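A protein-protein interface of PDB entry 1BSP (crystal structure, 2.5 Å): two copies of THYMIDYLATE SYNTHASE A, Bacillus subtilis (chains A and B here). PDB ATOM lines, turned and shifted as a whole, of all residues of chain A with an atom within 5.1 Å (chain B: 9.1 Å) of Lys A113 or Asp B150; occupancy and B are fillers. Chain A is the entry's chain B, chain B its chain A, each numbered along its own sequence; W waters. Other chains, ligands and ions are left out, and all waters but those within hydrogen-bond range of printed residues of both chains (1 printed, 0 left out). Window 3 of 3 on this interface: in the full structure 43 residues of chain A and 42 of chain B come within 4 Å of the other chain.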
ATOM      1  N   GLY A 108       9.541 -34.968 -19.341  1.00  0.00           N
ATOM      2  CA  GLY A 108       8.862 -34.409 -20.493  1.00  0.00           C
ATOM      3  C   GLY A 108       7.384 -34.169 -20.313  1.00  0.00           C
ATOM      4  O   GLY A 108       6.847 -33.215 -20.877  1.00  0.00           O
ATOM      5  N   PHE A 109       6.724 -35.017 -19.528  1.00  0.00           N
ATOM      6  CA  PHE A 109       5.292 -34.862 -19.292  1.00  0.00           C
ATOM      7  C   PHE A 109       4.993 -33.545 -18.581  1.00  0.00           C
ATOM      8  O   PHE A 109       4.011 -32.870 -18.894  1.00  0.00           O
ATOM      9  CB  PHE A 109       4.746 -36.016 -18.465  1.00  0.00           C
ATOM     10  CG  PHE A 109       3.270 -35.918 -18.197  1.00  0.00           C
ATOM     11  CD1 PHE A 109       2.351 -36.431 -19.102  1.00  0.00           C
ATOM     12  CD2 PHE A 109       2.806 -35.330 -17.025  1.00  0.00           C
ATOM     13  CE1 PHE A 109       0.990 -36.364 -18.838  1.00  0.00           C
ATOM     14  CE2 PHE A 109       1.454 -35.257 -16.753  1.00  0.00           C
ATOM     15  CZ  PHE A 109       0.540 -35.776 -17.658  1.00  0.00           C
ATOM     16  N   GLN A 110       5.840 -33.181 -17.628  1.00  0.00           N
ATOM     17  CA  GLN A 110       5.650 -31.938 -16.902  1.00  0.00           C
ATOM     18  C   GLN A 110       5.877 -30.745 -17.841  1.00  0.00           C
ATOM     19  O   GLN A 110       5.065 -29.814 -17.886  1.00  0.00           O
ATOM     20  CB  GLN A 110       6.596 -31.868 -15.698  1.00  0.00           C
ATOM     21  CG  GLN A 110       6.240 -32.827 -14.572  1.00  0.00           C
ATOM     22  CD  GLN A 110       4.807 -32.661 -14.106  1.00  0.00           C
ATOM     23  OE1 GLN A 110       4.337 -31.548 -13.903  1.00  0.00           O
ATOM     24  NE2 GLN A 110       4.105 -33.770 -13.934  1.00  0.00           N
ATOM     25  N   LEU A 111       6.950 -30.806 -18.623  1.00  0.00           N
ATOM     26  CA  LEU A 111       7.275 -29.733 -19.553  1.00  0.00           C
ATOM     27  C   LEU A 111       6.241 -29.557 -20.664  1.00  0.00           C
ATOM     28  O   LEU A 111       6.127 -28.475 -21.246  1.00  0.00           O
ATOM     29  CB  LEU A 111       8.663 -29.946 -20.159  1.00  0.00           C
ATOM     30  CG  LEU A 111       9.841 -29.824 -19.192  1.00  0.00           C
ATOM     31  CD1 LEU A 111      11.148 -30.055 -19.934  1.00  0.00           C
ATOM     32  CD2 LEU A 111       9.833 -28.455 -18.507  1.00  0.00           C
ATOM     33  N   GLY A 112       5.484 -30.609 -20.947  1.00  0.00           N
ATOM     34  CA  GLY A 112       4.486 -30.521 -21.992  1.00  0.00           C
ATOM     35  C   GLY A 112       3.079 -30.319 -21.478  1.00  0.00           C
ATOM     36  O   GLY A 112       2.126 -30.340 -22.255  1.00  0.00           O
ATOM     37  N   LYS A 113       2.925 -30.144 -20.170  1.00  0.00           N
ATOM     38  CA  LYS A 113       1.601 -29.938 -19.598  1.00  0.00           C
ATOM     39  C   LYS A 113       1.166 -28.490 -19.852  1.00  0.00           C
ATOM     40  O   LYS A 113       1.839 -27.544 -19.422  1.00  0.00           O
ATOM     41  CB  LYS A 113       1.624 -30.251 -18.102  1.00  0.00           C
ATOM     42  CG  LYS A 113       0.533 -31.199 -17.668  1.00  0.00           C
ATOM     43  CD  LYS A 113       0.535 -31.417 -16.161  1.00  0.00           C
ATOM     44  CE  LYS A 113      -0.646 -32.272 -15.749  1.00  0.00           C
ATOM     45  NZ  LYS A 113      -0.919 -32.172 -14.285  1.00  0.00           N
ATOM     46  N   LYS A 114       0.067 -28.320 -20.585  1.00  0.00           N
ATOM     47  CA  LYS A 114      -0.455 -26.987 -20.906  1.00  0.00           C
ATOM     48  C   LYS A 114      -1.195 -26.413 -19.695  1.00  0.00           C
ATOM     49  O   LYS A 114      -2.406 -26.570 -19.537  1.00  0.00           O
ATOM     50  CB  LYS A 114      -1.346 -27.042 -22.158  1.00  0.00           C
ATOM     51  CG  LYS A 114      -2.452 -28.088 -22.119  1.00  0.00           C
ATOM     52  CD  LYS A 114      -3.158 -28.230 -23.469  1.00  0.00           C
ATOM     53  CE  LYS A 114      -4.316 -29.225 -23.365  1.00  0.00           C
ATOM     54  NZ  LYS A 114      -4.929 -29.623 -24.668  1.00  0.00           N
ATOM     55  N   ASN A 115      -0.437 -25.740 -18.838  1.00  0.00           N
ATOM     56  CA  ASN A 115      -0.979 -25.187 -17.610  1.00  0.00           C
ATOM     57  C   ASN A 115      -0.852 -23.677 -17.388  1.00  0.00           C
ATOM     58  O   ASN A 115      -1.274 -23.172 -16.350  1.00  0.00           O
ATOM     59  CB  ASN A 115      -0.381 -25.934 -16.413  1.00  0.00           C
ATOM     60  CG  ASN A 115       1.117 -26.173 -16.554  1.00  0.00           C
ATOM     61  OD1 ASN A 115       1.599 -27.285 -16.346  1.00  0.00           O
ATOM     62  ND2 ASN A 115       1.858 -25.133 -16.917  1.00  0.00           N
ATOM     63  N   VAL A 123      -0.555 -22.551 -22.530  1.00  0.00           N
ATOM     64  CA  VAL A 123       0.732 -23.022 -23.034  1.00  0.00           C
ATOM     65  C   VAL A 123       1.459 -23.847 -21.976  1.00  0.00           C
ATOM     66  O   VAL A 123       0.992 -23.958 -20.834  1.00  0.00           O
ATOM     67  CB  VAL A 123       1.654 -21.851 -23.476  1.00  0.00           C
ATOM     68  CG1 VAL A 123       1.093 -21.174 -24.711  1.00  0.00           C
ATOM     69  CG2 VAL A 123       1.835 -20.849 -22.348  1.00  0.00           C
ATOM     70  N   ASP A 124       2.561 -24.480 -22.368  1.00  0.00           N
ATOM     71  CA  ASP A 124       3.347 -25.269 -21.423  1.00  0.00           C
ATOM     72  C   ASP A 124       4.560 -24.474 -20.949  1.00  0.00           C
ATOM     73  O   ASP A 124       4.864 -23.410 -21.490  1.00  0.00           O
ATOM     74  CB  ASP A 124       3.748 -26.631 -22.014  1.00  0.00           C
ATOM     75  CG  ASP A 124       4.532 -26.517 -23.312  1.00  0.00           C
ATOM     76  OD1 ASP A 124       5.585 -25.835 -23.337  1.00  0.00           O
ATOM     77  OD2 ASP A 124       4.105 -27.143 -24.305  1.00  0.00           O
ATOM     78  N   GLN A 125       5.265 -25.001 -19.957  1.00  0.00           N
ATOM     79  CA  GLN A 125       6.432 -24.329 -19.393  1.00  0.00           C
ATOM     80  C   GLN A 125       7.473 -23.879 -20.402  1.00  0.00           C
ATOM     81  O   GLN A 125       8.142 -22.868 -20.192  1.00  0.00           O
ATOM     82  CB  GLN A 125       7.114 -25.210 -18.346  1.00  0.00           C
ATOM     83  CG  GLN A 125       6.340 -25.363 -17.060  1.00  0.00           C
ATOM     84  CD  GLN A 125       7.099 -26.182 -16.044  1.00  0.00           C
ATOM     85  OE1 GLN A 125       8.185 -25.799 -15.621  1.00  0.00           O
ATOM     86  NE2 GLN A 125       6.551 -27.331 -15.676  1.00  0.00           N
ATOM     87  N   ASN A 148       6.834 -31.556  -9.687  1.00  0.00           N
ATOM     88  CA  ASN A 148       5.432 -31.204  -9.459  1.00  0.00           C
ATOM     89  C   ASN A 148       4.948 -31.973  -8.227  1.00  0.00           C
ATOM     90  O   ASN A 148       4.803 -33.196  -8.267  1.00  0.00           O
ATOM     91  CB  ASN A 148       4.582 -31.558 -10.679  1.00  0.00           C
ATOM     92  CG  ASN A 148       3.145 -31.108 -10.537  1.00  0.00           C
ATOM     93  OD1 ASN A 148       2.619 -31.004  -9.429  1.00  0.00           O
ATOM     94  ND2 ASN A 148       2.500 -30.831 -11.658  1.00  0.00           N
ATOM     95  N   ASP A 150       2.033 -32.420  -6.873  1.00  0.00           N
ATOM     96  CA  ASP A 150       0.823 -33.215  -7.086  1.00  0.00           C
ATOM     97  C   ASP A 150       1.060 -34.506  -7.860  1.00  0.00           C
ATOM     98  O   ASP A 150       0.330 -35.488  -7.694  1.00  0.00           O
ATOM     99  CB  ASP A 150      -0.223 -32.395  -7.854  1.00  0.00           C
ATOM    100  CG  ASP A 150      -0.804 -31.259  -7.040  1.00  0.00           C
ATOM    101  OD1 ASP A 150      -1.096 -31.467  -5.843  1.00  0.00           O
ATOM    102  OD2 ASP A 150      -0.994 -30.162  -7.610  1.00  0.00           O
ATOM    103  N   GLU A 151       2.075 -34.483  -8.718  1.00  0.00           N
ATOM    104  CA  GLU A 151       2.398 -35.610  -9.585  1.00  0.00           C
ATOM    105  C   GLU A 151       3.453 -36.591  -9.071  1.00  0.00           C
ATOM    106  O   GLU A 151       3.629 -37.667  -9.633  1.00  0.00           O
ATOM    107  CB  GLU A 151       2.821 -35.065 -10.951  1.00  0.00           C
ATOM    108  CG  GLU A 151       1.745 -34.247 -11.648  1.00  0.00           C
ATOM    109  CD  GLU A 151       0.715 -35.116 -12.355  1.00  0.00           C
ATOM    110  OE1 GLU A 151       0.370 -36.205 -11.847  1.00  0.00           O
ATOM    111  OE2 GLU A 151       0.257 -34.717 -13.440  1.00  0.00           O
ATOM    112  N   HIS B 105      -4.124 -19.983  -4.483  1.00  0.00           N
ATOM    113  CA  HIS B 105      -3.607 -21.300  -4.157  1.00  0.00           C
ATOM    114  C   HIS B 105      -2.099 -21.238  -3.924  1.00  0.00           C
ATOM    115  O   HIS B 105      -1.348 -22.079  -4.414  1.00  0.00           O
ATOM    116  CB  HIS B 105      -3.940 -22.267  -5.289  1.00  0.00           C
ATOM    117  CG  HIS B 105      -5.390 -22.638  -5.354  1.00  0.00           C
ATOM    118  ND1 HIS B 105      -5.929 -23.364  -6.392  1.00  0.00           N
ATOM    119  CD2 HIS B 105      -6.405 -22.416  -4.484  1.00  0.00           C
ATOM    120  CE1 HIS B 105      -7.212 -23.582  -6.160  1.00  0.00           C
ATOM    121  NE2 HIS B 105      -7.525 -23.017  -5.007  1.00  0.00           N
ATOM    122  N   GLN B 110      -0.409 -24.826  -0.670  1.00  0.00           N
ATOM    123  CA  GLN B 110       0.400 -25.900  -1.258  1.00  0.00           C
ATOM    124  C   GLN B 110       0.844 -26.930  -0.229  1.00  0.00           C
ATOM    125  O   GLN B 110       0.767 -28.133  -0.472  1.00  0.00           O
ATOM    126  CB  GLN B 110       1.636 -25.331  -1.972  1.00  0.00           C
ATOM    127  CG  GLN B 110       1.326 -24.650  -3.283  1.00  0.00           C
ATOM    128  CD  GLN B 110       0.454 -25.509  -4.181  1.00  0.00           C
ATOM    129  OE1 GLN B 110       0.709 -26.702  -4.370  1.00  0.00           O
ATOM    130  NE2 GLN B 110      -0.586 -24.906  -4.736  1.00  0.00           N
ATOM    131  N   LYS B 113      -2.058 -29.411   0.766  1.00  0.00           N
ATOM    132  CA  LYS B 113      -2.690 -30.325  -0.190  1.00  0.00           C
ATOM    133  C   LYS B 113      -2.326 -31.774   0.128  1.00  0.00           C
ATOM    134  O   LYS B 113      -1.150 -32.110   0.244  1.00  0.00           O
ATOM    135  CB  LYS B 113      -2.239 -30.014  -1.621  1.00  0.00           C
ATOM    136  CG  LYS B 113      -2.491 -28.603  -2.104  1.00  0.00           C
ATOM    137  CD  LYS B 113      -2.230 -28.493  -3.602  1.00  0.00           C
ATOM    138  CE  LYS B 113      -3.197 -29.381  -4.373  1.00  0.00           C
ATOM    139  NZ  LYS B 113      -3.127 -29.176  -5.842  1.00  0.00           N
ATOM    140  N   LEU B 146       6.796 -25.144  -3.132  1.00  0.00           N
ATOM    141  CA  LEU B 146       5.690 -24.198  -3.207  1.00  0.00           C
ATOM    142  C   LEU B 146       5.398 -23.837  -4.667  1.00  0.00           C
ATOM    143  O   LEU B 146       4.250 -23.584  -5.028  1.00  0.00           O
ATOM    144  CB  LEU B 146       5.984 -22.940  -2.388  1.00  0.00           C
ATOM    145  CG  LEU B 146       5.916 -23.093  -0.862  1.00  0.00           C
ATOM    146  CD1 LEU B 146       6.312 -21.793  -0.200  1.00  0.00           C
ATOM    147  CD2 LEU B 146       4.511 -23.502  -0.428  1.00  0.00           C
ATOM    148  N   TRP B 147       6.425 -23.877  -5.515  1.00  0.00           N
ATOM    149  CA  TRP B 147       6.278 -23.553  -6.936  1.00  0.00           C
ATOM    150  C   TRP B 147       5.555 -24.650  -7.723  1.00  0.00           C
ATOM    151  O   TRP B 147       6.174 -25.404  -8.462  1.00  0.00           O
ATOM    152  CB  TRP B 147       7.654 -23.265  -7.567  1.00  0.00           C
ATOM    153  CG  TRP B 147       7.592 -22.571  -8.922  1.00  0.00           C
ATOM    154  CD1 TRP B 147       7.449 -23.166 -10.146  1.00  0.00           C
ATOM    155  CD2 TRP B 147       7.624 -21.155  -9.170  1.00  0.00           C
ATOM    156  NE1 TRP B 147       7.380 -22.213 -11.134  1.00  0.00           N
ATOM    157  CE2 TRP B 147       7.482 -20.970 -10.566  1.00  0.00           C
ATOM    158  CE3 TRP B 147       7.752 -20.023  -8.350  1.00  0.00           C
ATOM    159  CZ2 TRP B 147       7.464 -19.700 -11.157  1.00  0.00           C
ATOM    160  CZ3 TRP B 147       7.735 -18.755  -8.944  1.00  0.00           C
ATOM    161  CH2 TRP B 147       7.591 -18.610 -10.333  1.00  0.00           C
ATOM    162  N   ASN B 148       4.244 -24.754  -7.549  1.00  0.00           N
ATOM    163  CA  ASN B 148       3.458 -25.756  -8.265  1.00  0.00           C
ATOM    164  C   ASN B 148       3.113 -25.200  -9.646  1.00  0.00           C
ATOM    165  O   ASN B 148       2.248 -24.332  -9.783  1.00  0.00           O
ATOM    166  CB  ASN B 148       2.183 -26.086  -7.494  1.00  0.00           C
ATOM    167  CG  ASN B 148       1.466 -27.298  -8.051  1.00  0.00           C
ATOM    168  OD1 ASN B 148       1.216 -27.394  -9.257  1.00  0.00           O
ATOM    169  ND2 ASN B 148       1.131 -28.233  -7.176  1.00  0.00           N
ATOM    170  N   PRO B 149       3.740 -25.742 -10.700  1.00  0.00           N
ATOM    171  CA  PRO B 149       3.502 -25.284 -12.071  1.00  0.00           C
ATOM    172  C   PRO B 149       2.058 -25.366 -12.566  1.00  0.00           C
ATOM    173  O   PRO B 149       1.632 -24.536 -13.366  1.00  0.00           O
ATOM    174  CB  PRO B 149       4.451 -26.161 -12.887  1.00  0.00           C
ATOM    175  CG  PRO B 149       4.454 -27.440 -12.123  1.00  0.00           C
ATOM    176  CD  PRO B 149       4.592 -26.946 -10.696  1.00  0.00           C
ATOM    177  N   ASP B 150       1.302 -26.342 -12.077  1.00  0.00           N
ATOM    178  CA  ASP B 150      -0.090 -26.508 -12.489  1.00  0.00           C
ATOM    179  C   ASP B 150      -1.031 -25.463 -11.921  1.00  0.00           C
ATOM    180  O   ASP B 150      -2.195 -25.421 -12.315  1.00  0.00           O
ATOM    181  CB  ASP B 150      -0.625 -27.881 -12.071  1.00  0.00           C
ATOM    182  CG  ASP B 150      -0.141 -28.997 -12.958  1.00  0.00           C
ATOM    183  OD1 ASP B 150       0.208 -28.724 -14.125  1.00  0.00           O
ATOM    184  OD2 ASP B 150      -0.121 -30.156 -12.494  1.00  0.00           O
ATOM    185  N   GLU B 151      -0.568 -24.671 -10.954  1.00  0.00           N
ATOM    186  CA  GLU B 151      -1.440 -23.673 -10.341  1.00  0.00           C
ATOM    187  C   GLU B 151      -0.854 -22.278 -10.183  1.00  0.00           C
ATOM    188  O   GLU B 151      -1.421 -21.457  -9.464  1.00  0.00           O
ATOM    189  CB  GLU B 151      -1.953 -24.171  -8.980  1.00  0.00           C
ATOM    190  CG  GLU B 151      -2.799 -25.433  -9.056  1.00  0.00           C
ATOM    191  CD  GLU B 151      -3.403 -25.833  -7.722  1.00  0.00           C
ATOM    192  OE1 GLU B 151      -2.647 -26.087  -6.756  1.00  0.00           O
ATOM    193  OE2 GLU B 151      -4.647 -25.905  -7.642  1.00  0.00           O
ATOM    194  N   LEU B 152       0.240 -21.985 -10.880  1.00  0.00           N
ATOM    195  CA  LEU B 152       0.873 -20.668 -10.783  1.00  0.00           C
ATOM    196  C   LEU B 152      -0.106 -19.524 -11.065  1.00  0.00           C
ATOM    197  O   LEU B 152       0.004 -18.446 -10.488  1.00  0.00           O
ATOM    198  CB  LEU B 152       2.069 -20.563 -11.731  1.00  0.00           C
ATOM    199  CG  LEU B 152       3.327 -21.355 -11.385  1.00  0.00           C
ATOM    200  CD1 LEU B 152       4.289 -21.322 -12.555  1.00  0.00           C
ATOM    201  CD2 LEU B 152       3.982 -20.802 -10.132  1.00  0.00           C
ATOM    202  N   ASP B 153      -1.068 -19.773 -11.946  1.00  0.00           N
ATOM    203  CA  ASP B 153      -2.056 -18.763 -12.289  1.00  0.00           C
ATOM    204  C   ASP B 153      -3.047 -18.522 -11.174  1.00  0.00           C
ATOM    205  O   ASP B 153      -3.616 -17.435 -11.070  1.00  0.00           O
ATOM    206  CB  ASP B 153      -2.836 -19.171 -13.536  1.00  0.00           C
ATOM    207  CG  ASP B 153      -2.004 -19.096 -14.795  1.00  0.00           C
ATOM    208  OD1 ASP B 153      -1.013 -18.325 -14.817  1.00  0.00           O
ATOM    209  OD2 ASP B 153      -2.357 -19.802 -15.767  1.00  0.00           O
ATOM    210  N   ALA B 154      -3.287 -19.548 -10.367  1.00  0.00           N
ATOM    211  CA  ALA B 154      -4.248 -19.439  -9.280  1.00  0.00           C
ATOM    212  C   ALA B 154      -3.636 -18.859  -8.015  1.00  0.00           C
ATOM    213  O   ALA B 154      -4.254 -18.903  -6.959  1.00  0.00           O
ATOM    214  CB  ALA B 154      -4.872 -20.800  -8.994  1.00  0.00           C
ATOM    215  N   MET B 155      -2.447 -18.283  -8.123  1.00  0.00           N
ATOM    216  CA  MET B 155      -1.786 -17.715  -6.960  1.00  0.00           C
ATOM    217  C   MET B 155      -1.785 -16.188  -6.984  1.00  0.00           C
ATOM    218  O   MET B 155      -1.201 -15.578  -7.882  1.00  0.00           O
ATOM    219  CB  MET B 155      -0.342 -18.223  -6.881  1.00  0.00           C
ATOM    220  CG  MET B 155      -0.194 -19.734  -6.754  1.00  0.00           C
ATOM    221  SD  MET B 155       1.538 -20.235  -6.671  1.00  0.00           S
ATOM    222  CE  MET B 155       1.378 -21.994  -7.109  1.00  0.00           C
HETATM  223  O   HOH W   1      -1.605 -30.529 -10.150  1.00  0.00           O
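The side-chain amino group (NZ) of Lys B113 lies within salt-bridge range of the side-chain carboxylate (OD2) of Asp A150, at 2.9 Å. ND2 of Asn B148 lies within hydrogen-bond range of OD2 of Asp A150 (2.9 Å). OD2 of Asp B150 is in salt-bridge range of NZ of Lys A113, 2.8 Å away. The side-chain carboxylate (OD1) of Asp B150 sits close to the side-chain amide oxygen (OD1) of Asn A115 (3.0 Å). The side-chain amide nitrogen (ND2) of Asn A148 sits at hydrogen-bond distance from the side-chain carboxylate (OD2) of Asp B150, at 2.8 Å.
The side-chain amide nitrogen of Asn B148 sits at hydrogen-bond distance from the side-chain amide oxygen of Gln B110, at 3.2 Å. The side-chain amino group (NZ) of Lys B113 lies within salt-bridge range of the side-chain carboxylate (OE1) of Glu B151, at 3.3 Å. The side-chain amide oxygen (OD1) of Asn B148 sits at hydrogen-bond distance from the backbone NH (N) of Asp B150 (3.0 Å). OE1 of Gln A110 lies within hydrogen-bond range of ND2 of Asn A148, 3.0 Å away. The side-chain amino group (NZ) of Lys A113 is in salt-bridge range of the side-chain carboxylate (OE2) of Glu A151 (2.9 Å). O of Val A123 is in hydrogen-bond range of N of Asn A115, at 3.0 Å.
Among the printed residues, merely in contact across the chains: Asn A115 with Asp B153, Asn A115 with Pro B149, Gln A125 with Pro B149, Asn A148 with Asn B148 and Asn A148 with Pro B149.
No residue of chain B comes within 4 Å of Gly A112. Lys A113 touches just one residue of chain B: Asp B150 (2.8 Å). Printed residues of chain B within 4 Å of Gln A125: Pro B149 (3.7 Å). Of the printed residues of chain B, Asn A148 touches Asn B148 (3.9 Å), Pro B149 (3.9 Å) and Asp B150 (2.8 Å). Of the printed residues of chain A, Lys B113 touches Asp A150 (2.9 Å). Asp B150 touches just these residues of chain A: Lys A113, Asn A115 and Asn A148. The nearest residue of chain B that does not touch Lys A113 is Pro B149 (6.8 Å). The nearest residue of chain A that does not touch Asp B150 is Glu A151 (4.6 Å).
Of the 13 printed residues of chain B, 5 touch a printed residue of chain A. Printed residues of chain B that touch a printed residue of chain A: Lys B113, Asn B148, Pro B149, Asp B150 and Asp B153. Of the 14 printed residues of chain A, 5 touch a printed residue of chain B.
Lys A113 touches Asp B150, and with the chains exchanged Asp A150 touches Lys B113. Asn A148 touches its own counterpart, Asn B148. Asn A148 touches Asp B150, and with the chains exchanged Asp A150 touches Asn B148. 5 positions are printed for both chains. Of the 10 pairs that touch across the chains among the printed residues, 5 have their exchanged pair printed and touching as well.
Water W1 bridges OD2 of Asp A150 (2.6 Å) and OD2 of Asp B150 (2.8 Å).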
